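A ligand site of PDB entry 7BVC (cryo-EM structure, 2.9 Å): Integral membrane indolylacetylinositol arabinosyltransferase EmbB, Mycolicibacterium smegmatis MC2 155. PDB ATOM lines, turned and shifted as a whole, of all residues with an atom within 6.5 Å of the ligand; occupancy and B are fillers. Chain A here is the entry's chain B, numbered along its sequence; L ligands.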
ATOM      1  N   SER A 284       6.968 -26.702  19.496  1.00  0.00           N
ATOM      2  CA  SER A 284       7.943 -27.771  19.616  1.00  0.00           C
ATOM      3  C   SER A 284       9.275 -27.312  20.183  1.00  0.00           C
ATOM      4  O   SER A 284       9.916 -28.064  20.930  1.00  0.00           O
ATOM      5  CB  SER A 284       8.184 -28.436  18.260  1.00  0.00           C
ATOM      6  OG  SER A 284       8.784 -27.543  17.352  1.00  0.00           O
ATOM      7  N   ASP A 285       9.712 -26.096  19.872  1.00  0.00           N
ATOM      8  CA  ASP A 285      10.981 -25.566  20.356  1.00  0.00           C
ATOM      9  C   ASP A 285      10.765 -24.677  21.583  1.00  0.00           C
ATOM     10  O   ASP A 285      11.130 -23.496  21.595  1.00  0.00           O
ATOM     11  CB  ASP A 285      11.704 -24.819  19.248  1.00  0.00           C
ATOM     12  CG  ASP A 285      12.172 -25.733  18.143  1.00  0.00           C
ATOM     13  OD1 ASP A 285      12.463 -26.918  18.435  1.00  0.00           O
ATOM     14  OD2 ASP A 285      12.248 -25.288  16.985  1.00  0.00           O
ATOM     15  N   TYR A 288      13.944 -26.121  23.995  1.00  0.00           N
ATOM     16  CA  TYR A 288      15.185 -25.655  23.337  1.00  0.00           C
ATOM     17  C   TYR A 288      15.502 -24.213  23.785  1.00  0.00           C
ATOM     18  O   TYR A 288      16.672 -23.955  24.155  1.00  0.00           O
ATOM     19  CB  TYR A 288      15.048 -25.739  21.806  1.00  0.00           C
ATOM     20  CG  TYR A 288      16.353 -25.711  21.056  1.00  0.00           C
ATOM     21  CD1 TYR A 288      16.918 -26.875  20.565  1.00  0.00           C
ATOM     22  CD2 TYR A 288      17.032 -24.517  20.839  1.00  0.00           C
ATOM     23  CE1 TYR A 288      18.119 -26.859  19.863  1.00  0.00           C
ATOM     24  CE2 TYR A 288      18.223 -24.489  20.146  1.00  0.00           C
ATOM     25  CZ  TYR A 288      18.770 -25.664  19.660  1.00  0.00           C
ATOM     26  OH  TYR A 288      19.953 -25.639  18.972  1.00  0.00           O
ATOM     27  N   ILE A 289      14.509 -23.327  23.736  1.00  0.00           N
ATOM     28  CA  ILE A 289      14.704 -21.932  24.128  1.00  0.00           C
ATOM     29  C   ILE A 289      14.797 -21.794  25.642  1.00  0.00           C
ATOM     30  O   ILE A 289      15.559 -20.951  26.145  1.00  0.00           O
ATOM     31  CB  ILE A 289      13.566 -21.067  23.546  1.00  0.00           C
ATOM     32  CG1 ILE A 289      13.553 -21.190  22.022  1.00  0.00           C
ATOM     33  CG2 ILE A 289      13.723 -19.617  23.962  1.00  0.00           C
ATOM     34  CD1 ILE A 289      12.558 -20.292  21.353  1.00  0.00           C
ATOM     35  N   MET A 292      18.250 -22.730  26.525  1.00  0.00           N
ATOM     36  CA  MET A 292      19.154 -21.691  26.051  1.00  0.00           C
ATOM     37  C   MET A 292      19.140 -20.480  26.981  1.00  0.00           C
ATOM     38  O   MET A 292      20.178 -19.852  27.201  1.00  0.00           O
ATOM     39  CB  MET A 292      18.776 -21.267  24.632  1.00  0.00           C
ATOM     40  CG  MET A 292      19.123 -22.281  23.567  1.00  0.00           C
ATOM     41  SD  MET A 292      19.306 -21.522  21.942  1.00  0.00           S
ATOM     42  CE  MET A 292      18.093 -20.213  22.048  1.00  0.00           C
ATOM     43  N   ASN A 304      24.300 -21.095  21.807  1.00  0.00           N
ATOM     44  CA  ASN A 304      23.437 -22.162  21.320  1.00  0.00           C
ATOM     45  C   ASN A 304      23.825 -23.431  22.077  1.00  0.00           C
ATOM     46  O   ASN A 304      24.943 -23.931  21.923  1.00  0.00           O
ATOM     47  CB  ASN A 304      23.588 -22.341  19.814  1.00  0.00           C
ATOM     48  CG  ASN A 304      22.368 -22.974  19.185  1.00  0.00           C
ATOM     49  OD1 ASN A 304      22.143 -24.181  19.321  1.00  0.00           O
ATOM     50  ND2 ASN A 304      21.589 -22.180  18.480  1.00  0.00           N
ATOM     51  N   TRP A 308      26.565 -26.966  17.435  1.00  0.00           N
ATOM     52  CA  TRP A 308      27.450 -25.992  16.781  1.00  0.00           C
ATOM     53  C   TRP A 308      28.568 -25.509  17.699  1.00  0.00           C
ATOM     54  O   TRP A 308      28.899 -24.321  17.721  1.00  0.00           O
ATOM     55  CB  TRP A 308      26.657 -24.812  16.225  1.00  0.00           C
ATOM     56  CG  TRP A 308      25.837 -25.181  15.032  1.00  0.00           C
ATOM     57  CD1 TRP A 308      26.253 -25.888  13.943  1.00  0.00           C
ATOM     58  CD2 TRP A 308      24.444 -24.901  14.824  1.00  0.00           C
ATOM     59  NE1 TRP A 308      25.221 -26.043  13.061  1.00  0.00           N
ATOM     60  CE2 TRP A 308      24.100 -25.443  13.580  1.00  0.00           C
ATOM     61  CE3 TRP A 308      23.473 -24.231  15.571  1.00  0.00           C
ATOM     62  CZ2 TRP A 308      22.818 -25.343  13.062  1.00  0.00           C
ATOM     63  CZ3 TRP A 308      22.204 -24.135  15.052  1.00  0.00           C
ATOM     64  CH2 TRP A 308      21.879 -24.689  13.809  1.00  0.00           C
ATOM     65  N   GLU A 313      23.943 -17.010  19.235  1.00  0.00           N
ATOM     66  CA  GLU A 313      22.998 -16.507  18.259  1.00  0.00           C
ATOM     67  C   GLU A 313      23.599 -15.255  17.623  1.00  0.00           C
ATOM     68  O   GLU A 313      23.775 -14.237  18.305  1.00  0.00           O
ATOM     69  CB  GLU A 313      21.654 -16.202  18.910  1.00  0.00           C
ATOM     70  CG  GLU A 313      21.059 -17.379  19.664  1.00  0.00           C
ATOM     71  CD  GLU A 313      20.827 -18.571  18.763  1.00  0.00           C
ATOM     72  OE1 GLU A 313      21.571 -19.572  18.901  1.00  0.00           O
ATOM     73  OE2 GLU A 313      19.911 -18.525  17.924  1.00  0.00           O
ATOM     74  N   TYR A 320      15.874 -13.161  23.050  1.00  0.00           N
ATOM     75  CA  TYR A 320      16.106 -14.170  24.075  1.00  0.00           C
ATOM     76  C   TYR A 320      16.731 -13.592  25.338  1.00  0.00           C
ATOM     77  O   TYR A 320      16.621 -14.200  26.407  1.00  0.00           O
ATOM     78  CB  TYR A 320      16.981 -15.293  23.524  1.00  0.00           C
ATOM     79  CG  TYR A 320      16.406 -15.979  22.297  1.00  0.00           C
ATOM     80  CD1 TYR A 320      15.037 -16.063  22.108  1.00  0.00           C
ATOM     81  CD2 TYR A 320      17.234 -16.538  21.334  1.00  0.00           C
ATOM     82  CE1 TYR A 320      14.503 -16.685  21.007  1.00  0.00           C
ATOM     83  CE2 TYR A 320      16.707 -17.158  20.226  1.00  0.00           C
ATOM     84  CZ  TYR A 320      15.341 -17.224  20.064  1.00  0.00           C
ATOM     85  OH  TYR A 320      14.814 -17.844  18.956  1.00  0.00           O
ATOM     86  N   ARG A 389       8.479 -20.108  20.582  1.00  0.00           N
ATOM     87  CA  ARG A 389       8.986 -19.675  19.280  1.00  0.00           C
ATOM     88  C   ARG A 389       8.545 -18.242  19.014  1.00  0.00           C
ATOM     89  O   ARG A 389       7.394 -17.876  19.271  1.00  0.00           O
ATOM     90  CB  ARG A 389       8.463 -20.600  18.172  1.00  0.00           C
ATOM     91  CG  ARG A 389       9.171 -21.931  18.087  1.00  0.00           C
ATOM     92  CD  ARG A 389      10.562 -21.775  17.511  1.00  0.00           C
ATOM     93  NE  ARG A 389      10.529 -21.349  16.111  1.00  0.00           N
ATOM     94  CZ  ARG A 389      10.798 -22.149  15.083  1.00  0.00           C
ATOM     95  NH1 ARG A 389      11.123 -23.415  15.287  1.00  0.00           N
ATOM     96  NH2 ARG A 389      10.744 -21.674  13.840  1.00  0.00           N
ATOM     97  N   PRO A 390       9.443 -17.392  18.491  1.00  0.00           N
ATOM     98  CA  PRO A 390       9.141 -15.967  18.312  1.00  0.00           C
ATOM     99  C   PRO A 390       8.456 -15.656  16.993  1.00  0.00           C
ATOM    100  O   PRO A 390       8.933 -14.833  16.201  1.00  0.00           O
ATOM    101  CB  PRO A 390      10.523 -15.324  18.406  1.00  0.00           C
ATOM    102  CG  PRO A 390      11.427 -16.347  17.816  1.00  0.00           C
ATOM    103  CD  PRO A 390      10.841 -17.705  18.133  1.00  0.00           C
ATOM    104  N   GLN A 431      14.782 -12.820  14.349  1.00  0.00           N
ATOM    105  CA  GLN A 431      15.067 -14.076  13.671  1.00  0.00           C
ATOM    106  C   GLN A 431      15.300 -13.788  12.202  1.00  0.00           C
ATOM    107  O   GLN A 431      14.830 -12.760  11.693  1.00  0.00           O
ATOM    108  CB  GLN A 431      13.907 -15.073  13.844  1.00  0.00           C
ATOM    109  CG  GLN A 431      13.888 -15.788  15.181  1.00  0.00           C
ATOM    110  CD  GLN A 431      14.735 -17.040  15.186  1.00  0.00           C
ATOM    111  OE1 GLN A 431      14.269 -18.121  14.858  1.00  0.00           O
ATOM    112  NE2 GLN A 431      16.002 -16.889  15.553  1.00  0.00           N
ATOM    113  N   ARG A 495      27.869 -22.382  11.362  1.00  0.00           N
ATOM    114  CA  ARG A 495      26.491 -22.763  11.111  1.00  0.00           C
ATOM    115  C   ARG A 495      26.233 -23.060   9.643  1.00  0.00           C
ATOM    116  O   ARG A 495      25.392 -23.898   9.323  1.00  0.00           O
ATOM    117  CB  ARG A 495      25.545 -21.659  11.583  1.00  0.00           C
ATOM    118  CG  ARG A 495      25.565 -21.421  13.079  1.00  0.00           C
ATOM    119  CD  ARG A 495      24.823 -20.144  13.429  1.00  0.00           C
ATOM    120  NE  ARG A 495      24.669 -19.991  14.872  1.00  0.00           N
ATOM    121  CZ  ARG A 495      23.533 -20.226  15.519  1.00  0.00           C
ATOM    122  NH1 ARG A 495      22.455 -20.621  14.866  1.00  0.00           N
ATOM    123  NH2 ARG A 495      23.473 -20.057  16.840  1.00  0.00           N
ATOM    124  N   TRP A 578      10.994 -24.861   7.625  1.00  0.00           N
ATOM    125  CA  TRP A 578      10.109 -25.575   8.528  1.00  0.00           C
ATOM    126  C   TRP A 578       8.654 -25.193   8.267  1.00  0.00           C
ATOM    127  O   TRP A 578       8.354 -24.327   7.446  1.00  0.00           O
ATOM    128  CB  TRP A 578      10.460 -25.290   9.993  1.00  0.00           C
ATOM    129  CG  TRP A 578      11.888 -25.491  10.358  1.00  0.00           C
ATOM    130  CD1 TRP A 578      12.733 -24.561  10.898  1.00  0.00           C
ATOM    131  CD2 TRP A 578      12.651 -26.698  10.242  1.00  0.00           C
ATOM    132  NE1 TRP A 578      13.967 -25.117  11.113  1.00  0.00           N
ATOM    133  CE2 TRP A 578      13.946 -26.432  10.721  1.00  0.00           C
ATOM    134  CE3 TRP A 578      12.364 -27.986   9.776  1.00  0.00           C
ATOM    135  CZ2 TRP A 578      14.954 -27.391  10.744  1.00  0.00           C
ATOM    136  CZ3 TRP A 578      13.359 -28.940   9.802  1.00  0.00           C
ATOM    137  CH2 TRP A 578      14.643 -28.640  10.281  1.00  0.00           C
ATOM    138  N   HIS A 580       6.788 -24.361  11.084  1.00  0.00           N
ATOM    139  CA  HIS A 580       6.545 -23.359  12.109  1.00  0.00           C
ATOM    140  C   HIS A 580       6.545 -21.940  11.563  1.00  0.00           C
ATOM    141  O   HIS A 580       5.989 -21.044  12.208  1.00  0.00           O
ATOM    142  CB  HIS A 580       7.596 -23.476  13.219  1.00  0.00           C
ATOM    143  CG  HIS A 580       8.056 -24.877  13.488  1.00  0.00           C
ATOM    144  ND1 HIS A 580       7.286 -25.791  14.160  1.00  0.00           N
ATOM    145  CD2 HIS A 580       9.210 -25.509  13.179  1.00  0.00           C
ATOM    146  CE1 HIS A 580       7.940 -26.937  14.246  1.00  0.00           C
ATOM    147  NE2 HIS A 580       9.116 -26.787  13.663  1.00  0.00           N
ATOM    148  N   TRP A 633       2.393 -32.263  19.722  1.00  0.00           N
ATOM    149  CA  TRP A 633       3.830 -32.503  19.556  1.00  0.00           C
ATOM    150  C   TRP A 633       4.412 -33.470  20.589  1.00  0.00           C
ATOM    151  O   TRP A 633       4.811 -34.588  20.254  1.00  0.00           O
ATOM    152  CB  TRP A 633       4.585 -31.173  19.585  1.00  0.00           C
ATOM    153  CG  TRP A 633       4.865 -30.649  18.217  1.00  0.00           C
ATOM    154  CD1 TRP A 633       4.382 -29.491  17.661  1.00  0.00           C
ATOM    155  CD2 TRP A 633       5.675 -31.262  17.212  1.00  0.00           C
ATOM    156  NE1 TRP A 633       4.851 -29.358  16.376  1.00  0.00           N
ATOM    157  CE2 TRP A 633       5.644 -30.433  16.086  1.00  0.00           C
ATOM    158  CE3 TRP A 633       6.420 -32.441  17.167  1.00  0.00           C
ATOM    159  CZ2 TRP A 633       6.345 -30.736  14.919  1.00  0.00           C
ATOM    160  CZ3 TRP A 633       7.114 -32.746  16.005  1.00  0.00           C
ATOM    161  CH2 TRP A 633       7.063 -31.894  14.897  1.00  0.00           C
ATOM    162  N   TRP A 972      16.540 -31.408  23.838  1.00  0.00           N
ATOM    163  CA  TRP A 972      15.951 -30.124  23.494  1.00  0.00           C
ATOM    164  C   TRP A 972      14.434 -30.167  23.383  1.00  0.00           C
ATOM    165  O   TRP A 972      13.814 -29.121  23.154  1.00  0.00           O
ATOM    166  CB  TRP A 972      16.552 -29.594  22.183  1.00  0.00           C
ATOM    167  CG  TRP A 972      16.332 -30.468  20.995  1.00  0.00           C
ATOM    168  CD1 TRP A 972      17.213 -31.366  20.457  1.00  0.00           C
ATOM    169  CD2 TRP A 972      15.174 -30.506  20.150  1.00  0.00           C
ATOM    170  NE1 TRP A 972      16.666 -31.960  19.350  1.00  0.00           N
ATOM    171  CE2 TRP A 972      15.416 -31.453  19.146  1.00  0.00           C
ATOM    172  CE3 TRP A 972      13.950 -29.823  20.162  1.00  0.00           C
ATOM    173  CZ2 TRP A 972      14.478 -31.749  18.162  1.00  0.00           C
ATOM    174  CZ3 TRP A 972      13.025 -30.123  19.176  1.00  0.00           C
ATOM    175  CH2 TRP A 972      13.285 -31.072  18.194  1.00  0.00           C
ATOM    176  N   SER A1008      15.349 -37.585  15.981  1.00  0.00           N
ATOM    177  CA  SER A1008      15.319 -36.125  16.020  1.00  0.00           C
ATOM    178  C   SER A1008      16.289 -35.514  17.019  1.00  0.00           C
ATOM    179  O   SER A1008      16.856 -34.458  16.741  1.00  0.00           O
ATOM    180  CB  SER A1008      13.889 -35.646  16.320  1.00  0.00           C
ATOM    181  OG  SER A1008      13.478 -36.039  17.609  1.00  0.00           O
ATOM    182  N   TRP A1012      20.452 -34.599  16.207  1.00  0.00           N
ATOM    183  CA  TRP A1012      20.677 -33.156  16.329  1.00  0.00           C
ATOM    184  C   TRP A1012      21.834 -32.867  17.269  1.00  0.00           C
ATOM    185  O   TRP A1012      22.723 -32.076  16.942  1.00  0.00           O
ATOM    186  CB  TRP A1012      19.400 -32.474  16.815  1.00  0.00           C
ATOM    187  CG  TRP A1012      19.470 -30.982  16.845  1.00  0.00           C
ATOM    188  CD1 TRP A1012      19.765 -30.190  17.914  1.00  0.00           C
ATOM    189  CD2 TRP A1012      19.238 -30.089  15.742  1.00  0.00           C
ATOM    190  NE1 TRP A1012      19.741 -28.866  17.548  1.00  0.00           N
ATOM    191  CE2 TRP A1012      19.415 -28.779  16.226  1.00  0.00           C
ATOM    192  CE3 TRP A1012      18.894 -30.279  14.404  1.00  0.00           C
ATOM    193  CZ2 TRP A1012      19.261 -27.656  15.408  1.00  0.00           C
ATOM    194  CZ3 TRP A1012      18.738 -29.165  13.596  1.00  0.00           C
ATOM    195  CH2 TRP A1012      18.924 -27.879  14.099  1.00  0.00           C
HETATM  196  C1  LIG L   1      17.850 -22.574  17.200  1.00  0.00           C
HETATM  197  O1  LIG L   1      12.406 -28.470  14.544  1.00  0.00           O
HETATM  198  C2  LIG L   1      13.134 -27.386  15.050  1.00  0.00           C
HETATM  199  C3  LIG L   1      14.617 -27.762  15.069  1.00  0.00           C
HETATM  200  C4  LIG L   1      14.789 -29.165  15.603  1.00  0.00           C
HETATM  201  C5  LIG L   1      15.158 -30.172  14.520  1.00  0.00           C
HETATM  202  N1  LIG L   1      15.321 -26.853  15.953  1.00  0.00           N
HETATM  203  C6  LIG L   1      15.156 -25.495  15.475  1.00  0.00           C
HETATM  204  C7  LIG L   1      16.259 -24.591  16.031  1.00  0.00           C
HETATM  205  N2  LIG L   1      15.681 -23.678  16.998  1.00  0.00           N
HETATM  206  C8  LIG L   1      16.361 -22.397  16.948  1.00  0.00           C
HETATM  207  O2  LIG L   1      18.384 -21.317  17.499  1.00  0.00           O
HETATM  208  C9  LIG L   1      15.783 -21.493  18.043  1.00  0.00           C
HETATM  209  C10 LIG L   1      14.267 -21.338  17.931  1.00  0.00           C
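OD2 of Asp 285 lies within salt-bridge range of N1 of the ligand, 3.6 Å away.
O2 of the ligand is in hydrogen-bond range of OE2 of Glu 313 (3.2 Å).
The side-chain amide nitrogen of Asn 304 sits at hydrogen-bond distance from an oxygen (O2) of the ligand (3.5 Å).
The side-chain carboxylate (OD2) of Asp 285 is in salt-bridge range of the guanidinium group (NH1) of Arg 389, at 2.8 Å.
The side-chain amide nitrogen (ND2) of Asn 304 lies within hydrogen-bond range of the side-chain carboxylate (OE1) of Glu 313, at 2.6 Å.
NH2 of Arg 495 is in salt-bridge range of OE1 of Glu 313 (2.8 Å).
The side-chain amide oxygen (OD1) of Asn 304 lies within hydrogen-bond range of the side-chain hydroxyl (OH) of Tyr 288, at 2.7 Å.
ND2 of Asn 304 sits close to NH2 of Arg 495 (3.3 Å).
The backbone NH (N) of Tyr 288 sits at hydrogen-bond distance from the backbone carbonyl oxygen (O) of Trp 972 (3.1 Å).
Residues that only touch the ligand: Tyr 288 (3.5 Å), Ile 289 (3.97 Å), Tyr 320 (3.7 Å), Arg 389 (3.8 Å), His 580 (3.8 Å), Trp 972 (3.6 Å) and Trp 1012 (3.7 Å).
Hydrophobic or aromatic side chains that line the ligand: Tyr 288, Ile 289, Trp 972 and Trp 1012.
Of the 19 residues printed, 10 come within 4 Å of the ligand.
The nearest printed residue that does not touch the ligand is Trp 578 (4.4 Å).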
